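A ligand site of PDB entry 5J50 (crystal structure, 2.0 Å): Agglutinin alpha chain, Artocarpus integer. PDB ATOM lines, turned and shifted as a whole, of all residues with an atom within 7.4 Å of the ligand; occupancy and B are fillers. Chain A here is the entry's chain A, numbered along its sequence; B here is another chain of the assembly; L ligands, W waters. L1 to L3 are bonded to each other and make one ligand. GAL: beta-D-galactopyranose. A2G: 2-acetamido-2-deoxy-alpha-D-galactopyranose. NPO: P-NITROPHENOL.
An oxygen (O4) of A2G L2 lies within hydrogen-bond range of the side-chain carboxylate (OD1) of Asp 125 (2.8 Å).
OH of Tyr 78 lies close to OH of NPO L3, 3.5 Å away.
N of Trp 123 lies within hydrogen-bond range of O6 of A2G L2.
N of Gly 1 is in hydrogen-bond range of O3 of A2G L2 (2.9 Å).
An oxygen (O6) of A2G L2 sits at hydrogen-bond distance from the backbone carbonyl oxygen (O) of Trp 123 (3.1 Å).
N of Tyr 122 lies within hydrogen-bond range of O5 of A2G L2 (3.0 Å).
The backbone carbonyl oxygen (O) of Gly 121 lies within hydrogen-bond range of the backbone NH (N) of Phe 47.
OD2 of Asp 125 is in hydrogen-bond range of OG of Ser 119 (2.6 Å).
The backbone carbonyl oxygen (O) of Asp 125 is in hydrogen-bond range of the backbone NH (N) of Ala 16 of chain B (2.8 Å).
O of Tyr 122 is in hydrogen-bond range of OG of Ser 46, 2.7 Å away.
CE2 of Phe 47 touches C8 of A2G L2 (3.4 Å).
Ser 76 touches the ligand.
Val 80 touches the ligand.
CA of Gly 121 touches O4 of A2G L2 (3.4 Å).
Hydrophobic or aromatic side chains within 4 Å of the ligand: Phe 47, Tyr 78, Val 80, Tyr 122 and Trp 123.
The nearest printed residue that does not touch the ligand is Ala 16 of chain B (4.1 Å).
Water W5 bridges O6 of GAL L1 (2.6 Å) and N of Val 79 (3.1 Å).
Water W9 lies within hydrogen-bond range of an oxygen (O4) of GAL L1 and the backbone NH (N) of Gly 1.
Water W8 lies within hydrogen-bond range of an oxygen (O2) of NPO L3 (3.0 Å) and the backbone carbonyl oxygen (O) of Ser 76 (3.1 Å).
Water W6 lies within hydrogen-bond range of the side-chain hydroxyl of Tyr 122 (2.6 Å) and an oxygen (O2) of NPO L3 (3.0 Å).
Water W1 bridges N of Gly 1 (2.5 Å) and O2 of GAL L1 (3.0 Å).
Water W7 bridges the side-chain hydroxyl (OH) of Tyr 78 (2.9 Å) and a nitrogen (N2) of A2G L2 (3.2 Å).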
ATOM      1  N   GLY A   1      -3.987 -19.383 -19.154  1.00  0.00           N
ATOM      2  CA  GLY A   1      -3.628 -20.695 -19.764  1.00  0.00           C
ATOM      3  C   GLY A   1      -2.420 -21.353 -19.094  1.00  0.00           C
ATOM      4  O   GLY A   1      -1.907 -20.840 -18.110  1.00  0.00           O
ATOM      5  N   LYS A   2      -2.018 -22.512 -19.589  1.00  0.00           N
ATOM      6  CA  LYS A   2      -0.909 -23.238 -19.029  1.00  0.00           C
ATOM      7  C   LYS A   2       0.319 -22.853 -19.865  1.00  0.00           C
ATOM      8  O   LYS A   2       0.367 -23.131 -21.087  1.00  0.00           O
ATOM      9  CB  LYS A   2      -1.100 -24.753 -19.086  1.00  0.00           C
ATOM     10  CG  LYS A   2       0.046 -25.564 -18.478  1.00  0.00           C
ATOM     11  CD  LYS A   2      -0.234 -27.060 -18.598  1.00  0.00           C
ATOM     12  CE  LYS A   2       0.535 -27.789 -17.498  1.00  0.00           C
ATOM     13  NZ  LYS A   2       0.811 -29.291 -17.618  1.00  0.00           N
ATOM     14  N   ILE A  25      -5.860 -21.216 -33.103  1.00  0.00           N
ATOM     15  CA  ILE A  25      -4.928 -22.313 -32.997  1.00  0.00           C
ATOM     16  C   ILE A  25      -5.243 -22.967 -31.673  1.00  0.00           C
ATOM     17  O   ILE A  25      -5.533 -22.260 -30.672  1.00  0.00           O
ATOM     18  CB  ILE A  25      -3.437 -21.808 -32.996  1.00  0.00           C
ATOM     19  CG1 ILE A  25      -3.119 -21.062 -34.313  1.00  0.00           C
ATOM     20  CG2 ILE A  25      -2.486 -22.975 -32.796  1.00  0.00           C
ATOM     21  CD1 ILE A  25      -3.357 -21.894 -35.564  1.00  0.00           C
ATOM     22  N   SER A  46      -4.557 -27.821 -26.002  1.00  0.00           N
ATOM     23  CA  SER A  46      -5.644 -26.965 -25.476  1.00  0.00           C
ATOM     24  C   SER A  46      -6.430 -27.627 -24.302  1.00  0.00           C
ATOM     25  O   SER A  46      -6.457 -28.842 -24.173  1.00  0.00           O
ATOM     26  CB  SER A  46      -6.588 -26.623 -26.584  1.00  0.00           C
ATOM     27  OG  SER A  46      -7.846 -26.240 -26.083  1.00  0.00           O
ATOM     28  N   PHE A  47      -7.138 -26.839 -23.494  1.00  0.00           N
ATOM     29  CA  PHE A  47      -7.987 -27.391 -22.403  1.00  0.00           C
ATOM     30  C   PHE A  47      -9.118 -28.161 -23.018  1.00  0.00           C
ATOM     31  O   PHE A  47      -9.595 -29.120 -22.442  1.00  0.00           O
ATOM     32  CB  PHE A  47      -8.562 -26.304 -21.453  1.00  0.00           C
ATOM     33  CG  PHE A  47      -7.524 -25.482 -20.705  1.00  0.00           C
ATOM     34  CD1 PHE A  47      -6.186 -25.854 -20.670  1.00  0.00           C
ATOM     35  CD2 PHE A  47      -7.901 -24.343 -20.032  1.00  0.00           C
ATOM     36  CE1 PHE A  47      -5.239 -25.104 -19.991  1.00  0.00           C
ATOM     37  CE2 PHE A  47      -6.994 -23.590 -19.336  1.00  0.00           C
ATOM     38  CZ  PHE A  47      -5.644 -23.962 -19.313  1.00  0.00           C
ATOM     39  N   ILE A  48      -9.524 -27.754 -24.219  1.00  0.00           N
ATOM     40  CA  ILE A  48     -10.620 -28.403 -24.893  1.00  0.00           C
ATOM     41  C   ILE A  48     -10.126 -29.197 -26.112  1.00  0.00           C
ATOM     42  O   ILE A  48      -8.987 -29.097 -26.515  1.00  0.00           O
ATOM     43  CB  ILE A  48     -11.741 -27.416 -25.259  1.00  0.00           C
ATOM     44  CG1 ILE A  48     -11.241 -26.298 -26.174  1.00  0.00           C
ATOM     45  CG2 ILE A  48     -12.351 -26.776 -24.011  1.00  0.00           C
ATOM     46  CD1 ILE A  48     -12.379 -25.609 -26.905  1.00  0.00           C
ATOM     47  N   VAL A  75     -11.115 -13.975 -28.996  1.00  0.00           N
ATOM     48  CA  VAL A  75     -12.075 -15.101 -29.027  1.00  0.00           C
ATOM     49  C   VAL A  75     -12.714 -15.328 -27.633  1.00  0.00           C
ATOM     50  O   VAL A  75     -11.998 -15.526 -26.647  1.00  0.00           O
ATOM     51  CB  VAL A  75     -11.417 -16.393 -29.517  1.00  0.00           C
ATOM     52  CG1 VAL A  75     -12.443 -17.533 -29.547  1.00  0.00           C
ATOM     53  CG2 VAL A  75     -10.840 -16.202 -30.922  1.00  0.00           C
ATOM     54  N   SER A  76     -14.048 -15.256 -27.539  1.00  0.00           N
ATOM     55  CA  SER A  76     -14.747 -15.315 -26.234  1.00  0.00           C
ATOM     56  C   SER A  76     -14.155 -14.381 -25.152  1.00  0.00           C
ATOM     57  O   SER A  76     -14.166 -14.701 -23.981  1.00  0.00           O
ATOM     58  CB  SER A  76     -14.680 -16.734 -25.658  1.00  0.00           C
ATOM     59  OG  SER A  76     -15.203 -17.658 -26.539  1.00  0.00           O
ATOM     60  N   GLY A  77     -13.609 -13.246 -25.554  1.00  0.00           N
ATOM     61  CA  GLY A  77     -13.146 -12.257 -24.607  1.00  0.00           C
ATOM     62  C   GLY A  77     -11.665 -12.401 -24.306  1.00  0.00           C
ATOM     63  O   GLY A  77     -11.130 -11.713 -23.445  1.00  0.00           O
ATOM     64  N   TYR A  78     -11.005 -13.304 -25.012  1.00  0.00           N
ATOM     65  CA  TYR A  78      -9.560 -13.458 -24.858  1.00  0.00           C
ATOM     66  C   TYR A  78      -8.769 -13.078 -26.094  1.00  0.00           C
ATOM     67  O   TYR A  78      -9.201 -13.348 -27.228  1.00  0.00           O
ATOM     68  CB  TYR A  78      -9.229 -14.893 -24.484  1.00  0.00           C
ATOM     69  CG  TYR A  78      -9.895 -15.280 -23.230  1.00  0.00           C
ATOM     70  CD1 TYR A  78     -11.211 -15.759 -23.240  1.00  0.00           C
ATOM     71  CD2 TYR A  78      -9.243 -15.101 -22.000  1.00  0.00           C
ATOM     72  CE1 TYR A  78     -11.851 -16.080 -22.068  1.00  0.00           C
ATOM     73  CE2 TYR A  78      -9.873 -15.460 -20.801  1.00  0.00           C
ATOM     74  CZ  TYR A  78     -11.178 -15.959 -20.856  1.00  0.00           C
ATOM     75  OH  TYR A  78     -11.825 -16.336 -19.697  1.00  0.00           O
ATOM     76  N   VAL A  79      -7.604 -12.496 -25.865  1.00  0.00           N
ATOM     77  CA  VAL A  79      -6.676 -12.273 -26.954  1.00  0.00           C
ATOM     78  C   VAL A  79      -5.931 -13.562 -27.134  1.00  0.00           C
ATOM     79  O   VAL A  79      -5.275 -14.051 -26.179  1.00  0.00           O
ATOM     80  CB  VAL A  79      -5.683 -11.101 -26.651  1.00  0.00           C
ATOM     81  CG1 VAL A  79      -4.643 -10.967 -27.757  1.00  0.00           C
ATOM     82  CG2 VAL A  79      -6.488  -9.796 -26.530  1.00  0.00           C
ATOM     83  N   VAL A  80      -6.012 -14.106 -28.342  1.00  0.00           N
ATOM     84  CA  VAL A  80      -5.320 -15.353 -28.671  1.00  0.00           C
ATOM     85  C   VAL A  80      -4.660 -15.365 -30.035  1.00  0.00           C
ATOM     86  O   VAL A  80      -4.919 -14.439 -30.857  1.00  0.00           O
ATOM     87  CB  VAL A  80      -6.266 -16.582 -28.540  1.00  0.00           C
ATOM     88  CG1 VAL A  80      -6.822 -16.713 -27.093  1.00  0.00           C
ATOM     89  CG2 VAL A  80      -7.331 -16.538 -29.576  1.00  0.00           C
ATOM     90  N   SER A 119       1.975 -20.037 -24.085  1.00  0.00           N
ATOM     91  CA  SER A 119       0.912 -20.491 -23.222  1.00  0.00           C
ATOM     92  C   SER A 119      -0.338 -20.906 -23.984  1.00  0.00           C
ATOM     93  O   SER A 119      -0.682 -20.350 -25.042  1.00  0.00           O
ATOM     94  CB  SER A 119       0.614 -19.438 -22.163  1.00  0.00           C
ATOM     95  OG  SER A 119      -0.601 -19.649 -21.530  1.00  0.00           O
ATOM     96  N   ILE A 120      -1.052 -21.888 -23.468  1.00  0.00           N
ATOM     97  CA  ILE A 120      -2.272 -22.375 -24.149  1.00  0.00           C
ATOM     98  C   ILE A 120      -3.340 -22.624 -23.107  1.00  0.00           C
ATOM     99  O   ILE A 120      -3.060 -23.186 -22.079  1.00  0.00           O
ATOM    100  CB  ILE A 120      -2.014 -23.619 -25.022  1.00  0.00           C
ATOM    101  CG1 ILE A 120      -0.940 -23.269 -26.087  1.00  0.00           C
ATOM    102  CG2 ILE A 120      -3.286 -24.151 -25.696  1.00  0.00           C
ATOM    103  CD1 ILE A 120      -0.420 -24.453 -26.860  1.00  0.00           C
ATOM    104  N   GLY A 121      -4.528 -22.071 -23.350  1.00  0.00           N
ATOM    105  CA  GLY A 121      -5.668 -22.211 -22.471  1.00  0.00           C
ATOM    106  C   GLY A 121      -6.646 -22.968 -23.348  1.00  0.00           C
ATOM    107  O   GLY A 121      -6.345 -24.116 -23.732  1.00  0.00           O
ATOM    108  N   TYR A 122      -7.792 -22.365 -23.666  1.00  0.00           N
ATOM    109  CA  TYR A 122      -8.646 -22.918 -24.714  1.00  0.00           C
ATOM    110  C   TYR A 122      -8.002 -22.821 -26.097  1.00  0.00           C
ATOM    111  O   TYR A 122      -8.246 -23.701 -26.974  1.00  0.00           O
ATOM    112  CB  TYR A 122      -9.985 -22.253 -24.778  1.00  0.00           C
ATOM    113  CG  TYR A 122     -11.017 -22.773 -23.794  1.00  0.00           C
ATOM    114  CD1 TYR A 122     -10.684 -22.995 -22.454  1.00  0.00           C
ATOM    115  CD2 TYR A 122     -12.343 -22.952 -24.188  1.00  0.00           C
ATOM    116  CE1 TYR A 122     -11.616 -23.457 -21.545  1.00  0.00           C
ATOM    117  CE2 TYR A 122     -13.310 -23.384 -23.250  1.00  0.00           C
ATOM    118  CZ  TYR A 122     -12.914 -23.653 -21.935  1.00  0.00           C
ATOM    119  OH  TYR A 122     -13.780 -24.052 -21.013  1.00  0.00           O
ATOM    120  N   TRP A 123      -7.199 -21.773 -26.288  1.00  0.00           N
ATOM    121  CA  TRP A 123      -6.427 -21.570 -27.503  1.00  0.00           C
ATOM    122  C   TRP A 123      -5.018 -21.140 -27.167  1.00  0.00           C
ATOM    123  O   TRP A 123      -4.718 -20.771 -26.022  1.00  0.00           O
ATOM    124  CB  TRP A 123      -7.120 -20.487 -28.327  1.00  0.00           C
ATOM    125  CG  TRP A 123      -8.538 -20.907 -28.559  1.00  0.00           C
ATOM    126  CD1 TRP A 123      -8.974 -21.884 -29.408  1.00  0.00           C
ATOM    127  CD2 TRP A 123      -9.777 -20.399 -27.899  1.00  0.00           C
ATOM    128  NE1 TRP A 123     -10.330 -22.036 -29.326  1.00  0.00           N
ATOM    129  CE2 TRP A 123     -10.883 -21.190 -28.450  1.00  0.00           C
ATOM    130  CE3 TRP A 123     -10.046 -19.452 -26.904  1.00  0.00           C
ATOM    131  CZ2 TRP A 123     -12.212 -21.015 -28.033  1.00  0.00           C
ATOM    132  CZ3 TRP A 123     -11.386 -19.283 -26.506  1.00  0.00           C
ATOM    133  CH2 TRP A 123     -12.440 -20.057 -27.054  1.00  0.00           C
ATOM    134  N   LEU A 124      -4.140 -21.158 -28.173  1.00  0.00           N
ATOM    135  CA  LEU A 124      -2.784 -20.598 -28.032  1.00  0.00           C
ATOM    136  C   LEU A 124      -2.907 -19.104 -27.675  1.00  0.00           C
ATOM    137  O   LEU A 124      -3.435 -18.313 -28.519  1.00  0.00           O
ATOM    138  CB  LEU A 124      -1.948 -20.854 -29.303  1.00  0.00           C
ATOM    139  CG  LEU A 124      -0.555 -20.215 -29.498  1.00  0.00           C
ATOM    140  CD1 LEU A 124       0.460 -20.887 -28.581  1.00  0.00           C
ATOM    141  CD2 LEU A 124      -0.088 -20.259 -30.952  1.00  0.00           C
ATOM    142  N   ASP A 125      -2.445 -18.748 -26.469  1.00  0.00           N
ATOM    143  CA  ASP A 125      -2.554 -17.386 -25.930  1.00  0.00           C
ATOM    144  C   ASP A 125      -1.515 -16.485 -26.603  1.00  0.00           C
ATOM    145  O   ASP A 125      -1.872 -15.475 -27.217  1.00  0.00           O
ATOM    146  CB  ASP A 125      -2.343 -17.328 -24.416  1.00  0.00           C
ATOM    147  CG  ASP A 125      -3.311 -18.220 -23.643  1.00  0.00           C
ATOM    148  OD1 ASP A 125      -4.509 -18.166 -23.972  1.00  0.00           O
ATOM    149  OD2 ASP A 125      -2.854 -18.978 -22.733  1.00  0.00           O
ATOM    150  N   TYR A 126      -0.258 -16.904 -26.475  1.00  0.00           N
ATOM    151  CA  TYR A 126       0.926 -16.292 -27.082  1.00  0.00           C
ATOM    152  C   TYR A 126       2.032 -17.354 -27.260  1.00  0.00           C
ATOM    153  O   TYR A 126       1.953 -18.479 -26.717  1.00  0.00           O
ATOM    154  CB  TYR A 126       1.409 -15.106 -26.237  1.00  0.00           C
ATOM    155  CG  TYR A 126       1.652 -15.488 -24.801  1.00  0.00           C
ATOM    156  CD1 TYR A 126       2.870 -16.053 -24.391  1.00  0.00           C
ATOM    157  CD2 TYR A 126       0.647 -15.311 -23.851  1.00  0.00           C
ATOM    158  CE1 TYR A 126       3.057 -16.451 -23.089  1.00  0.00           C
ATOM    159  CE2 TYR A 126       0.833 -15.674 -22.536  1.00  0.00           C
ATOM    160  CZ  TYR A 126       2.051 -16.230 -22.167  1.00  0.00           C
ATOM    161  OH  TYR A 126       2.239 -16.608 -20.832  1.00  0.00           O
ATOM    162  N   ALA B  16      -1.615 -12.788 -26.607  1.00  0.00           N
ATOM    163  CA  ALA B  16      -1.966 -12.102 -25.382  1.00  0.00           C
ATOM    164  C   ALA B  16      -0.732 -11.504 -24.675  1.00  0.00           C
ATOM    165  O   ALA B  16       0.202 -12.222 -24.205  1.00  0.00           O
ATOM    166  CB  ALA B  16      -2.790 -12.954 -24.439  1.00  0.00           C
ATOM    167  N   LYS B  17      -0.753 -10.173 -24.624  1.00  0.00           N
ATOM    168  CA  LYS B  17       0.267  -9.379 -23.996  1.00  0.00           C
ATOM    169  C   LYS B  17       0.031  -9.440 -22.460  1.00  0.00           C
ATOM    170  O   LYS B  17       0.656 -10.241 -21.746  1.00  0.00           O
ATOM    171  CB  LYS B  17       0.159  -7.936 -24.532  1.00  0.00           C
HETATM  172  C1  GAL L   1      -6.535 -16.494 -18.763  1.00  0.00           C
HETATM  173  C2  GAL L   1      -5.729 -16.338 -17.512  1.00  0.00           C
HETATM  174  C3  GAL L   1      -5.452 -14.884 -17.159  1.00  0.00           C
HETATM  175  C4  GAL L   1      -4.881 -14.142 -18.359  1.00  0.00           C
HETATM  176  C5  GAL L   1      -5.715 -14.432 -19.697  1.00  0.00           C
HETATM  177  C6  GAL L   1      -4.975 -13.989 -20.929  1.00  0.00           C
HETATM  178  O2  GAL L   1      -6.437 -17.021 -16.496  1.00  0.00           O
HETATM  179  O3  GAL L   1      -4.397 -14.870 -16.127  1.00  0.00           O
HETATM  180  O4  GAL L   1      -3.516 -14.566 -18.577  1.00  0.00           O
HETATM  181  O5  GAL L   1      -5.897 -15.863 -19.861  1.00  0.00           O
HETATM  182  O6  GAL L   1      -5.929 -13.657 -21.975  1.00  0.00           O
HETATM  183  O5  A2G L   2      -8.474 -19.897 -22.137  1.00  0.00           O
HETATM  184  C1  A2G L   2      -8.984 -20.094 -20.877  1.00  0.00           C
HETATM  185  C2  A2G L   2      -7.933 -19.692 -19.897  1.00  0.00           C
HETATM  186  N2  A2G L   2      -8.566 -19.692 -18.620  1.00  0.00           N
HETATM  187  C3  A2G L   2      -7.505 -18.215 -20.100  1.00  0.00           C
HETATM  188  O3  A2G L   2      -6.495 -17.907 -19.140  1.00  0.00           O
HETATM  189  C4  A2G L   2      -6.972 -18.068 -21.521  1.00  0.00           C
HETATM  190  O4  A2G L   2      -5.853 -18.945 -21.605  1.00  0.00           O
HETATM  191  C5  A2G L   2      -8.144 -18.490 -22.440  1.00  0.00           C
HETATM  192  C6  A2G L   2      -7.770 -18.347 -23.903  1.00  0.00           C
HETATM  193  O6  A2G L   2      -7.104 -19.539 -24.398  1.00  0.00           O
HETATM  194  C7  A2G L   2      -8.016 -20.129 -17.520  1.00  0.00           C
HETATM  195  O7  A2G L   2      -8.712 -20.058 -16.379  1.00  0.00           O
HETATM  196  C8  A2G L   2      -6.588 -20.745 -17.468  1.00  0.00           C
HETATM  197  C1  NPO L   3     -13.953 -19.910 -22.346  1.00  0.00           C
HETATM  198  C2  NPO L   3     -12.818 -19.772 -23.174  1.00  0.00           C
HETATM  199  C3  NPO L   3     -11.552 -19.575 -22.605  1.00  0.00           C
HETATM  200  C4  NPO L   3     -11.389 -19.492 -21.201  1.00  0.00           C
HETATM  201  C5  NPO L   3     -12.522 -19.587 -20.381  1.00  0.00           C
HETATM  202  C6  NPO L   3     -13.783 -19.791 -20.962  1.00  0.00           C
HETATM  203  OH  NPO L   3     -10.139 -19.229 -20.634  1.00  0.00           O
HETATM  204  N1  NPO L   3     -15.198 -20.160 -22.893  1.00  0.00           N
HETATM  205  O2  NPO L   3     -16.309 -20.011 -22.150  1.00  0.00           O
HETATM  206  O3  NPO L   3     -15.356 -20.598 -24.323  1.00  0.00           O
HETATM  207  O   HOH W   1      -4.132 -18.981 -16.662  1.00  0.00           O
HETATM  208  O   HOH W   2      -5.429 -15.626 -23.821  1.00  0.00           O
HETATM  209  O   HOH W   3      -4.804 -22.717 -15.716  1.00  0.00           O
HETATM  210  O   HOH W   4      -1.562 -13.603 -17.292  1.00  0.00           O
HETATM  211  O   HOH W   5      -6.760 -11.458 -23.027  1.00  0.00           O
HETATM  212  O   HOH W   6     -15.998 -22.984 -21.988  1.00  0.00           O
HETATM  213  O   HOH W   7     -10.619 -17.539 -17.396  1.00  0.00           O
HETATM  214  O   HOH W   8     -15.448 -17.241 -22.703  1.00  0.00           O
HETATM  215  O   HOH W   9      -2.793 -16.933 -19.821  1.00  0.00           O
